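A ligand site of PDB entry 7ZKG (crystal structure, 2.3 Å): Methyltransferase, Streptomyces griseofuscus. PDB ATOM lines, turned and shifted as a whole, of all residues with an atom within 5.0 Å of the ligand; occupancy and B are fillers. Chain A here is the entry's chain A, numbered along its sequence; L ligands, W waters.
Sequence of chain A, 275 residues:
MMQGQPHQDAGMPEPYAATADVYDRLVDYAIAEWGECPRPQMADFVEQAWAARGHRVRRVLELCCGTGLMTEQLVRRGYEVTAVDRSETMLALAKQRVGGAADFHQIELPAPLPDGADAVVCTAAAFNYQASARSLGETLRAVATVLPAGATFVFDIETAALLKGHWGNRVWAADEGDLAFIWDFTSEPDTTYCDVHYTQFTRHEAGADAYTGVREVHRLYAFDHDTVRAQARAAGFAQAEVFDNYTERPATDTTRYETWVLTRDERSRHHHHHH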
ATOM      1  N   ARG A  39      26.408  32.261 -35.793  1.00  0.00           N
ATOM      2  CA  ARG A  39      25.573  32.292 -34.594  1.00  0.00           C
ATOM      3  C   ARG A  39      25.019  33.679 -34.290  1.00  0.00           C
ATOM      4  O   ARG A  39      23.860  33.786 -33.875  1.00  0.00           O
ATOM      5  CB  ARG A  39      26.362  31.744 -33.396  1.00  0.00           C
ATOM      6  CG  ARG A  39      26.904  30.342 -33.617  1.00  0.00           C
ATOM      7  CD  ARG A  39      25.859  29.423 -34.246  1.00  0.00           C
ATOM      8  NE  ARG A  39      26.297  28.029 -34.296  1.00  0.00           N
ATOM      9  CZ  ARG A  39      26.787  27.423 -35.373  1.00  0.00           C
ATOM     10  NH1 ARG A  39      26.922  28.068 -36.531  1.00  0.00           N
ATOM     11  NH2 ARG A  39      27.151  26.155 -35.296  1.00  0.00           N
ATOM     12  N   GLU A  62      18.179  26.438 -23.856  1.00  0.00           N
ATOM     13  CA  GLU A  62      18.884  26.065 -25.081  1.00  0.00           C
ATOM     14  C   GLU A  62      19.158  24.563 -25.067  1.00  0.00           C
ATOM     15  O   GLU A  62      19.805  24.053 -24.152  1.00  0.00           O
ATOM     16  CB  GLU A  62      20.203  26.832 -25.220  1.00  0.00           C
ATOM     17  CG  GLU A  62      20.941  26.468 -26.505  1.00  0.00           C
ATOM     18  CD  GLU A  62      22.388  26.896 -26.496  1.00  0.00           C
ATOM     19  OE1 GLU A  62      22.818  27.500 -25.491  1.00  0.00           O
ATOM     20  OE2 GLU A  62      23.088  26.632 -27.481  1.00  0.00           O
ATOM     21  N   LEU A  63      18.667  23.878 -26.094  1.00  0.00           N
ATOM     22  CA  LEU A  63      18.869  22.437 -26.232  1.00  0.00           C
ATOM     23  C   LEU A  63      20.111  22.171 -27.071  1.00  0.00           C
ATOM     24  O   LEU A  63      20.372  22.858 -28.065  1.00  0.00           O
ATOM     25  CB  LEU A  63      17.663  21.776 -26.881  1.00  0.00           C
ATOM     26  CG  LEU A  63      16.288  22.073 -26.281  1.00  0.00           C
ATOM     27  CD1 LEU A  63      15.221  21.240 -26.976  1.00  0.00           C
ATOM     28  CD2 LEU A  63      16.268  21.809 -24.784  1.00  0.00           C
ATOM     29  N   CYS A  64      20.871  21.150 -26.670  1.00  0.00           N
ATOM     30  CA  CYS A  64      22.052  20.677 -27.399  1.00  0.00           C
ATOM     31  C   CYS A  64      23.025  21.833 -27.660  1.00  0.00           C
ATOM     32  O   CYS A  64      23.306  22.202 -28.799  1.00  0.00           O
ATOM     33  CB  CYS A  64      21.637  20.008 -28.703  1.00  0.00           C
ATOM     34  SG  CYS A  64      20.380  18.713 -28.524  1.00  0.00           S
ATOM     35  N   CYS A  65      23.538  22.397 -26.563  1.00  0.00           N
ATOM     36  CA  CYS A  65      24.351  23.603 -26.655  1.00  0.00           C
ATOM     37  C   CYS A  65      25.732  23.338 -27.237  1.00  0.00           C
ATOM     38  O   CYS A  65      26.378  24.284 -27.703  1.00  0.00           O
ATOM     39  CB  CYS A  65      24.480  24.263 -25.283  1.00  0.00           C
ATOM     40  SG  CYS A  65      25.287  23.243 -24.032  1.00  0.00           S
ATOM     41  N   GLY A  66      26.209  22.094 -27.216  1.00  0.00           N
ATOM     42  CA  GLY A  66      27.534  21.797 -27.732  1.00  0.00           C
ATOM     43  C   GLY A  66      28.600  22.599 -27.009  1.00  0.00           C
ATOM     44  O   GLY A  66      28.588  22.724 -25.773  1.00  0.00           O
ATOM     45  N   LEU A  69      28.453  28.033 -28.652  1.00  0.00           N
ATOM     46  CA  LEU A  69      28.528  29.210 -29.509  1.00  0.00           C
ATOM     47  C   LEU A  69      27.233  30.006 -29.464  1.00  0.00           C
ATOM     48  O   LEU A  69      27.257  31.240 -29.382  1.00  0.00           O
ATOM     49  CB  LEU A  69      28.869  28.804 -30.940  1.00  0.00           C
ATOM     50  CG  LEU A  69      30.319  28.399 -31.239  1.00  0.00           C
ATOM     51  CD1 LEU A  69      30.419  27.820 -32.632  1.00  0.00           C
ATOM     52  CD2 LEU A  69      31.255  29.587 -31.072  1.00  0.00           C
ATOM     53  N   MET A  70      26.086  29.328 -29.528  1.00  0.00           N
ATOM     54  CA  MET A  70      24.808  30.016 -29.387  1.00  0.00           C
ATOM     55  C   MET A  70      24.578  30.449 -27.939  1.00  0.00           C
ATOM     56  O   MET A  70      24.000  31.518 -27.687  1.00  0.00           O
ATOM     57  CB  MET A  70      23.663  29.124 -29.863  1.00  0.00           C
ATOM     58  CG  MET A  70      22.306  29.801 -29.874  1.00  0.00           C
ATOM     59  SD  MET A  70      22.211  31.170 -31.045  1.00  0.00           S
ATOM     60  CE  MET A  70      20.472  31.565 -30.945  1.00  0.00           C
ATOM     61  N   ASP A  85      22.861  19.481 -22.711  1.00  0.00           N
ATOM     62  CA  ASP A  85      23.593  18.654 -23.668  1.00  0.00           C
ATOM     63  C   ASP A  85      23.822  17.310 -23.011  1.00  0.00           C
ATOM     64  O   ASP A  85      23.915  17.214 -21.780  1.00  0.00           O
ATOM     65  CB  ASP A  85      24.915  19.303 -24.094  1.00  0.00           C
ATOM     66  CG  ASP A  85      25.465  18.724 -25.387  1.00  0.00           C
ATOM     67  OD1 ASP A  85      25.901  17.543 -25.381  1.00  0.00           O
ATOM     68  OD2 ASP A  85      25.448  19.431 -26.407  1.00  0.00           O
ATOM     69  N   ARG A  86      23.905  16.256 -23.822  1.00  0.00           N
ATOM     70  CA  ARG A  86      24.129  14.925 -23.273  1.00  0.00           C
ATOM     71  C   ARG A  86      25.574  14.682 -22.872  1.00  0.00           C
ATOM     72  O   ARG A  86      25.844  13.707 -22.153  1.00  0.00           O
ATOM     73  CB  ARG A  86      23.695  13.846 -24.257  1.00  0.00           C
ATOM     74  CG  ARG A  86      24.524  13.772 -25.522  1.00  0.00           C
ATOM     75  CD  ARG A  86      24.427  12.398 -26.178  1.00  0.00           C
ATOM     76  NE  ARG A  86      24.835  12.437 -27.573  1.00  0.00           N
ATOM     77  CZ  ARG A  86      24.037  12.148 -28.592  1.00  0.00           C
ATOM     78  NH1 ARG A  86      22.789  11.746 -28.412  1.00  0.00           N
ATOM     79  NH2 ARG A  86      24.499  12.278 -29.837  1.00  0.00           N
ATOM     80  N   SER A  87      26.501  15.537 -23.295  1.00  0.00           N
ATOM     81  CA  SER A  87      27.930  15.326 -23.093  1.00  0.00           C
ATOM     82  C   SER A  87      28.448  16.275 -22.022  1.00  0.00           C
ATOM     83  O   SER A  87      28.324  17.494 -22.165  1.00  0.00           O
ATOM     84  CB  SER A  87      28.691  15.527 -24.408  1.00  0.00           C
ATOM     85  OG  SER A  87      30.082  15.642 -24.172  1.00  0.00           O
ATOM     86  N   MET A  90      31.144  18.588 -23.588  1.00  0.00           N
ATOM     87  CA  MET A  90      30.624  19.805 -24.213  1.00  0.00           C
ATOM     88  C   MET A  90      30.192  20.826 -23.177  1.00  0.00           C
ATOM     89  O   MET A  90      30.492  22.022 -23.311  1.00  0.00           O
ATOM     90  CB  MET A  90      29.457  19.450 -25.137  1.00  0.00           C
ATOM     91  CG  MET A  90      29.844  18.651 -26.370  1.00  0.00           C
ATOM     92  SD  MET A  90      31.058  19.483 -27.410  1.00  0.00           S
ATOM     93  CE  MET A  90      30.595  18.843 -29.014  1.00  0.00           C
ATOM     94  N   ILE A 107      21.518  16.234 -20.040  1.00  0.00           N
ATOM     95  CA  ILE A 107      20.268  15.556 -20.350  1.00  0.00           C
ATOM     96  C   ILE A 107      20.402  14.883 -21.709  1.00  0.00           C
ATOM     97  O   ILE A 107      20.878  15.505 -22.665  1.00  0.00           O
ATOM     98  CB  ILE A 107      19.076  16.541 -20.358  1.00  0.00           C
ATOM     99  CG1 ILE A 107      18.915  17.226 -19.005  1.00  0.00           C
ATOM    100  CG2 ILE A 107      17.789  15.814 -20.723  1.00  0.00           C
ATOM    101  CD1 ILE A 107      17.931  18.369 -19.013  1.00  0.00           C
ATOM    102  N   GLU A 108      19.986  13.630 -21.795  1.00  0.00           N
ATOM    103  CA  GLU A 108      19.905  12.896 -23.059  1.00  0.00           C
ATOM    104  C   GLU A 108      18.470  12.992 -23.577  1.00  0.00           C
ATOM    105  O   GLU A 108      17.571  12.331 -23.056  1.00  0.00           O
ATOM    106  CB  GLU A 108      20.327  11.435 -22.871  1.00  0.00           C
ATOM    107  CG  GLU A 108      19.998  10.525 -24.054  1.00  0.00           C
ATOM    108  CD  GLU A 108      21.146  10.386 -25.035  1.00  0.00           C
ATOM    109  OE1 GLU A 108      22.290  10.178 -24.585  1.00  0.00           O
ATOM    110  OE2 GLU A 108      20.903  10.468 -26.270  1.00  0.00           O
ATOM    111  N   LEU A 109      18.268  13.807 -24.611  1.00  0.00           N
ATOM    112  CA  LEU A 109      16.943  14.033 -25.169  1.00  0.00           C
ATOM    113  C   LEU A 109      16.530  12.844 -26.036  1.00  0.00           C
ATOM    114  O   LEU A 109      17.362  12.276 -26.744  1.00  0.00           O
ATOM    115  CB  LEU A 109      16.918  15.313 -25.989  1.00  0.00           C
ATOM    116  CG  LEU A 109      17.281  16.594 -25.218  1.00  0.00           C
ATOM    117  CD1 LEU A 109      17.274  17.795 -26.142  1.00  0.00           C
ATOM    118  CD2 LEU A 109      16.333  16.795 -24.052  1.00  0.00           C
ATOM    119  N   PRO A 110      15.250  12.460 -26.031  1.00  0.00           N
ATOM    120  CA  PRO A 110      14.169  13.067 -25.238  1.00  0.00           C
ATOM    121  C   PRO A 110      14.113  12.611 -23.772  1.00  0.00           C
ATOM    122  O   PRO A 110      14.238  11.420 -23.472  1.00  0.00           O
ATOM    123  CB  PRO A 110      12.900  12.613 -25.972  1.00  0.00           C
ATOM    124  CG  PRO A 110      13.286  11.331 -26.608  1.00  0.00           C
ATOM    125  CD  PRO A 110      14.729  11.483 -27.001  1.00  0.00           C
ATOM    126  N   THR A 123      19.928  25.075 -31.985  1.00  0.00           N
ATOM    127  CA  THR A 123      20.561  25.545 -33.209  1.00  0.00           C
ATOM    128  C   THR A 123      21.591  24.546 -33.724  1.00  0.00           C
ATOM    129  O   THR A 123      22.047  23.650 -33.008  1.00  0.00           O
ATOM    130  CB  THR A 123      21.229  26.910 -32.992  1.00  0.00           C
ATOM    131  OG1 THR A 123      22.227  26.805 -31.968  1.00  0.00           O
ATOM    132  CG2 THR A 123      20.186  27.949 -32.570  1.00  0.00           C
ATOM    133  N   ALA A 124      21.952  24.726 -35.000  1.00  0.00           N
ATOM    134  CA  ALA A 124      23.022  23.992 -35.676  1.00  0.00           C
ATOM    135  C   ALA A 124      22.686  22.505 -35.810  1.00  0.00           C
ATOM    136  O   ALA A 124      23.506  21.628 -35.500  1.00  0.00           O
ATOM    137  CB  ALA A 124      24.361  24.193 -34.982  1.00  0.00           C
ATOM    138  N   ALA A 126      21.024  20.073 -34.533  1.00  0.00           N
ATOM    139  CA  ALA A 126      21.075  19.022 -33.531  1.00  0.00           C
ATOM    140  C   ALA A 126      19.971  17.990 -33.740  1.00  0.00           C
ATOM    141  O   ALA A 126      20.173  16.799 -33.470  1.00  0.00           O
ATOM    142  CB  ALA A 126      20.968  19.627 -32.123  1.00  0.00           C
ATOM    143  N   TYR A 129      20.160  14.486 -35.525  1.00  0.00           N
ATOM    144  CA  TYR A 129      20.662  13.311 -34.829  1.00  0.00           C
ATOM    145  C   TYR A 129      19.563  12.446 -34.248  1.00  0.00           C
ATOM    146  O   TYR A 129      19.829  11.310 -33.844  1.00  0.00           O
ATOM    147  CB  TYR A 129      21.634  13.728 -33.712  1.00  0.00           C
ATOM    148  CG  TYR A 129      22.965  14.215 -34.252  1.00  0.00           C
ATOM    149  CD1 TYR A 129      24.006  13.322 -34.489  1.00  0.00           C
ATOM    150  CD2 TYR A 129      23.170  15.560 -34.528  1.00  0.00           C
ATOM    151  CE1 TYR A 129      25.220  13.763 -34.980  1.00  0.00           C
ATOM    152  CE2 TYR A 129      24.379  16.010 -35.016  1.00  0.00           C
ATOM    153  CZ  TYR A 129      25.400  15.103 -35.237  1.00  0.00           C
ATOM    154  OH  TYR A 129      26.608  15.543 -35.736  1.00  0.00           O
ATOM    155  N   GLN A 130      18.322  12.946 -34.190  1.00  0.00           N
ATOM    156  CA  GLN A 130      17.188  12.100 -33.843  1.00  0.00           C
ATOM    157  C   GLN A 130      17.024  11.011 -34.894  1.00  0.00           C
ATOM    158  O   GLN A 130      16.773  11.300 -36.068  1.00  0.00           O
ATOM    159  CB  GLN A 130      15.917  12.941 -33.746  1.00  0.00           C
ATOM    160  CG  GLN A 130      16.017  14.112 -32.779  1.00  0.00           C
ATOM    161  CD  GLN A 130      16.126  13.685 -31.334  1.00  0.00           C
ATOM    162  OE1 GLN A 130      15.509  12.698 -30.922  1.00  0.00           O
ATOM    163  NE2 GLN A 130      16.916  14.407 -30.557  1.00  0.00           N
HETATM  164  N1  LIG L   1      24.077  24.338 -30.661  1.00  0.00           N
HETATM  165  C1  LIG L   1      25.464  24.128 -31.130  1.00  0.00           C
HETATM  166  C2  LIG L   1      25.601  22.861 -31.984  1.00  0.00           C
HETATM  167  C3  LIG L   1      25.362  21.578 -31.211  1.00  0.00           C
HETATM  168  S1  LIG L   1      24.846  20.160 -32.230  1.00  0.00           S
HETATM  169  C4  LIG L   1      25.931  25.335 -31.934  1.00  0.00           C
HETATM  170  O1  LIG L   1      27.027  25.404 -32.442  1.00  0.00           O
HETATM  171  O2  LIG L   1      25.029  26.284 -32.008  1.00  0.00           O
HETATM  172  C5  LIG L   1      25.812  18.797 -31.526  1.00  0.00           C
HETATM  173  C6  LIG L   1      25.603  18.771 -30.027  1.00  0.00           C
HETATM  174  O3  LIG L   1      24.301  18.246 -29.688  1.00  0.00           O
HETATM  175  C7  LIG L   1      26.631  17.889 -29.300  1.00  0.00           C
HETATM  176  O4  LIG L   1      27.188  18.560 -28.181  1.00  0.00           O
HETATM  177  C8  LIG L   1      25.814  16.656 -28.883  1.00  0.00           C
HETATM  178  O5  LIG L   1      26.294  16.101 -27.664  1.00  0.00           O
HETATM  179  C9  LIG L   1      24.437  17.269 -28.679  1.00  0.00           C
HETATM  180  N2  LIG L   1      23.339  16.318 -28.789  1.00  0.00           N
HETATM  181  C10 LIG L   1      23.001  15.564 -29.882  1.00  0.00           C
HETATM  182  N3  LIG L   1      21.972  14.778 -29.700  1.00  0.00           N
HETATM  183  C11 LIG L   1      21.595  15.038 -28.391  1.00  0.00           C
HETATM  184  C12 LIG L   1      20.562  14.523 -27.580  1.00  0.00           C
HETATM  185  N4  LIG L   1      19.688  13.585 -27.984  1.00  0.00           N
HETATM  186  N5  LIG L   1      20.455  14.984 -26.319  1.00  0.00           N
HETATM  187  C13 LIG L   1      21.331  15.909 -25.903  1.00  0.00           C
HETATM  188  N6  LIG L   1      22.345  16.469 -26.569  1.00  0.00           N
HETATM  189  C14 LIG L   1      22.422  15.980 -27.819  1.00  0.00           C
HETATM  190  O   HOH W   1      25.375  26.649 -28.518  1.00  0.00           O
HETATM  191  O   HOH W   2      21.667  25.304 -29.379  1.00  0.00           O
HETATM  192  O   HOH W   3      28.448  25.586 -30.124  1.00  0.00           O
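An oxygen (O4) of the ligand is in hydrogen-bond range of the side-chain carboxylate (OD2) of Asp 85 (2.6 Å).
O of Thr 123 is in hydrogen-bond range of N1 of the ligand (3.2 Å).
O2 of the ligand is in hydrogen-bond range of OG1 of Thr 123, at 2.9 Å.
A nitrogen (N1) of the ligand lies within hydrogen-bond range of the backbone carbonyl oxygen (O) of Cys 64 (2.9 Å).
The side-chain sulfur (SG) of Cys 64 sits close to a nitrogen (N6) of the ligand (3.6 Å).
A nitrogen (N5) of the ligand lies within hydrogen-bond range of the backbone NH of Leu 109.
A nitrogen (N4) of the ligand is in hydrogen-bond range of the backbone carbonyl oxygen (O) of Leu 109.
O1 of the ligand lies within salt-bridge range of NH2 of Arg 39.
N6 of the ligand is in hydrogen-bond range of N of Arg 86 (3.2 Å).
NH1 of Arg 86 is in hydrogen-bond range of N3 of the ligand, at 3.4 Å.
The side-chain carboxylate (OD2) of Asp 85 lies within hydrogen-bond range of the backbone NH (N) of Gly 66, 2.9 Å away.
O of Asp 85 lies within hydrogen-bond range of N of Ile 107 (3.1 Å).
The side-chain carboxylate (OD1) of Asp 85 is in hydrogen-bond range of the backbone NH (N) of Ser 87, 3.0 Å away.
The backbone carbonyl oxygen (O) of Ile 107 sits at hydrogen-bond distance from the backbone NH (N) of Arg 86, at 3.3 Å.
NH1 of Arg 86 lies within salt-bridge range of OE2 of Glu 108.
N of Met 90 is in hydrogen-bond range of OG of Ser 87, 3.2 Å away.
Water W3 lies within hydrogen-bond range of O1 of the ligand (2.7 Å), N of Leu 69 (2.9 Å) and O of Cys 65 (3.4 Å).
Water W2 lies within hydrogen-bond range of OE2 of Glu 62 (2.7 Å), N1 of the ligand (2.9 Å), OG1 of Thr 123 (3.0 Å) and O of Leu 63 (3.1 Å).
Water W1 lies within hydrogen-bond range of OE2 of Glu 62, O of Cys 65, N of Met 70, N of Leu 69 and N1 of the ligand.
Cys 65 touches the ligand (O to C1, 3.6 Å).
CA of Gly 66 touches O4 of the ligand, at 3.3 Å.
Met 70 touches the ligand.
CG of Met 90 touches O4 of the ligand (3.2 Å).
Ile 107 touches the ligand (O to C13, 3.3 Å).
Glu 108 touches the ligand (OE2 to N4, 3.8 Å).
CB of Ala 124 touches C2 of the ligand (3.5 Å).
Ala 126 touches the ligand (CB to S1, 3.9 Å).
Gln 130 touches the ligand (NE2 to N4, 3.9 Å).
Hydrophobic or aromatic side chains within 4 Å of the ligand: Met 70, Met 90, Leu 109, Ala 124 and Ala 126.
Of the 21 residues printed, 15 come within 4 Å of the ligand.
The nearest printed residue that does not touch the ligand is Glu 62 (4.04 Å).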
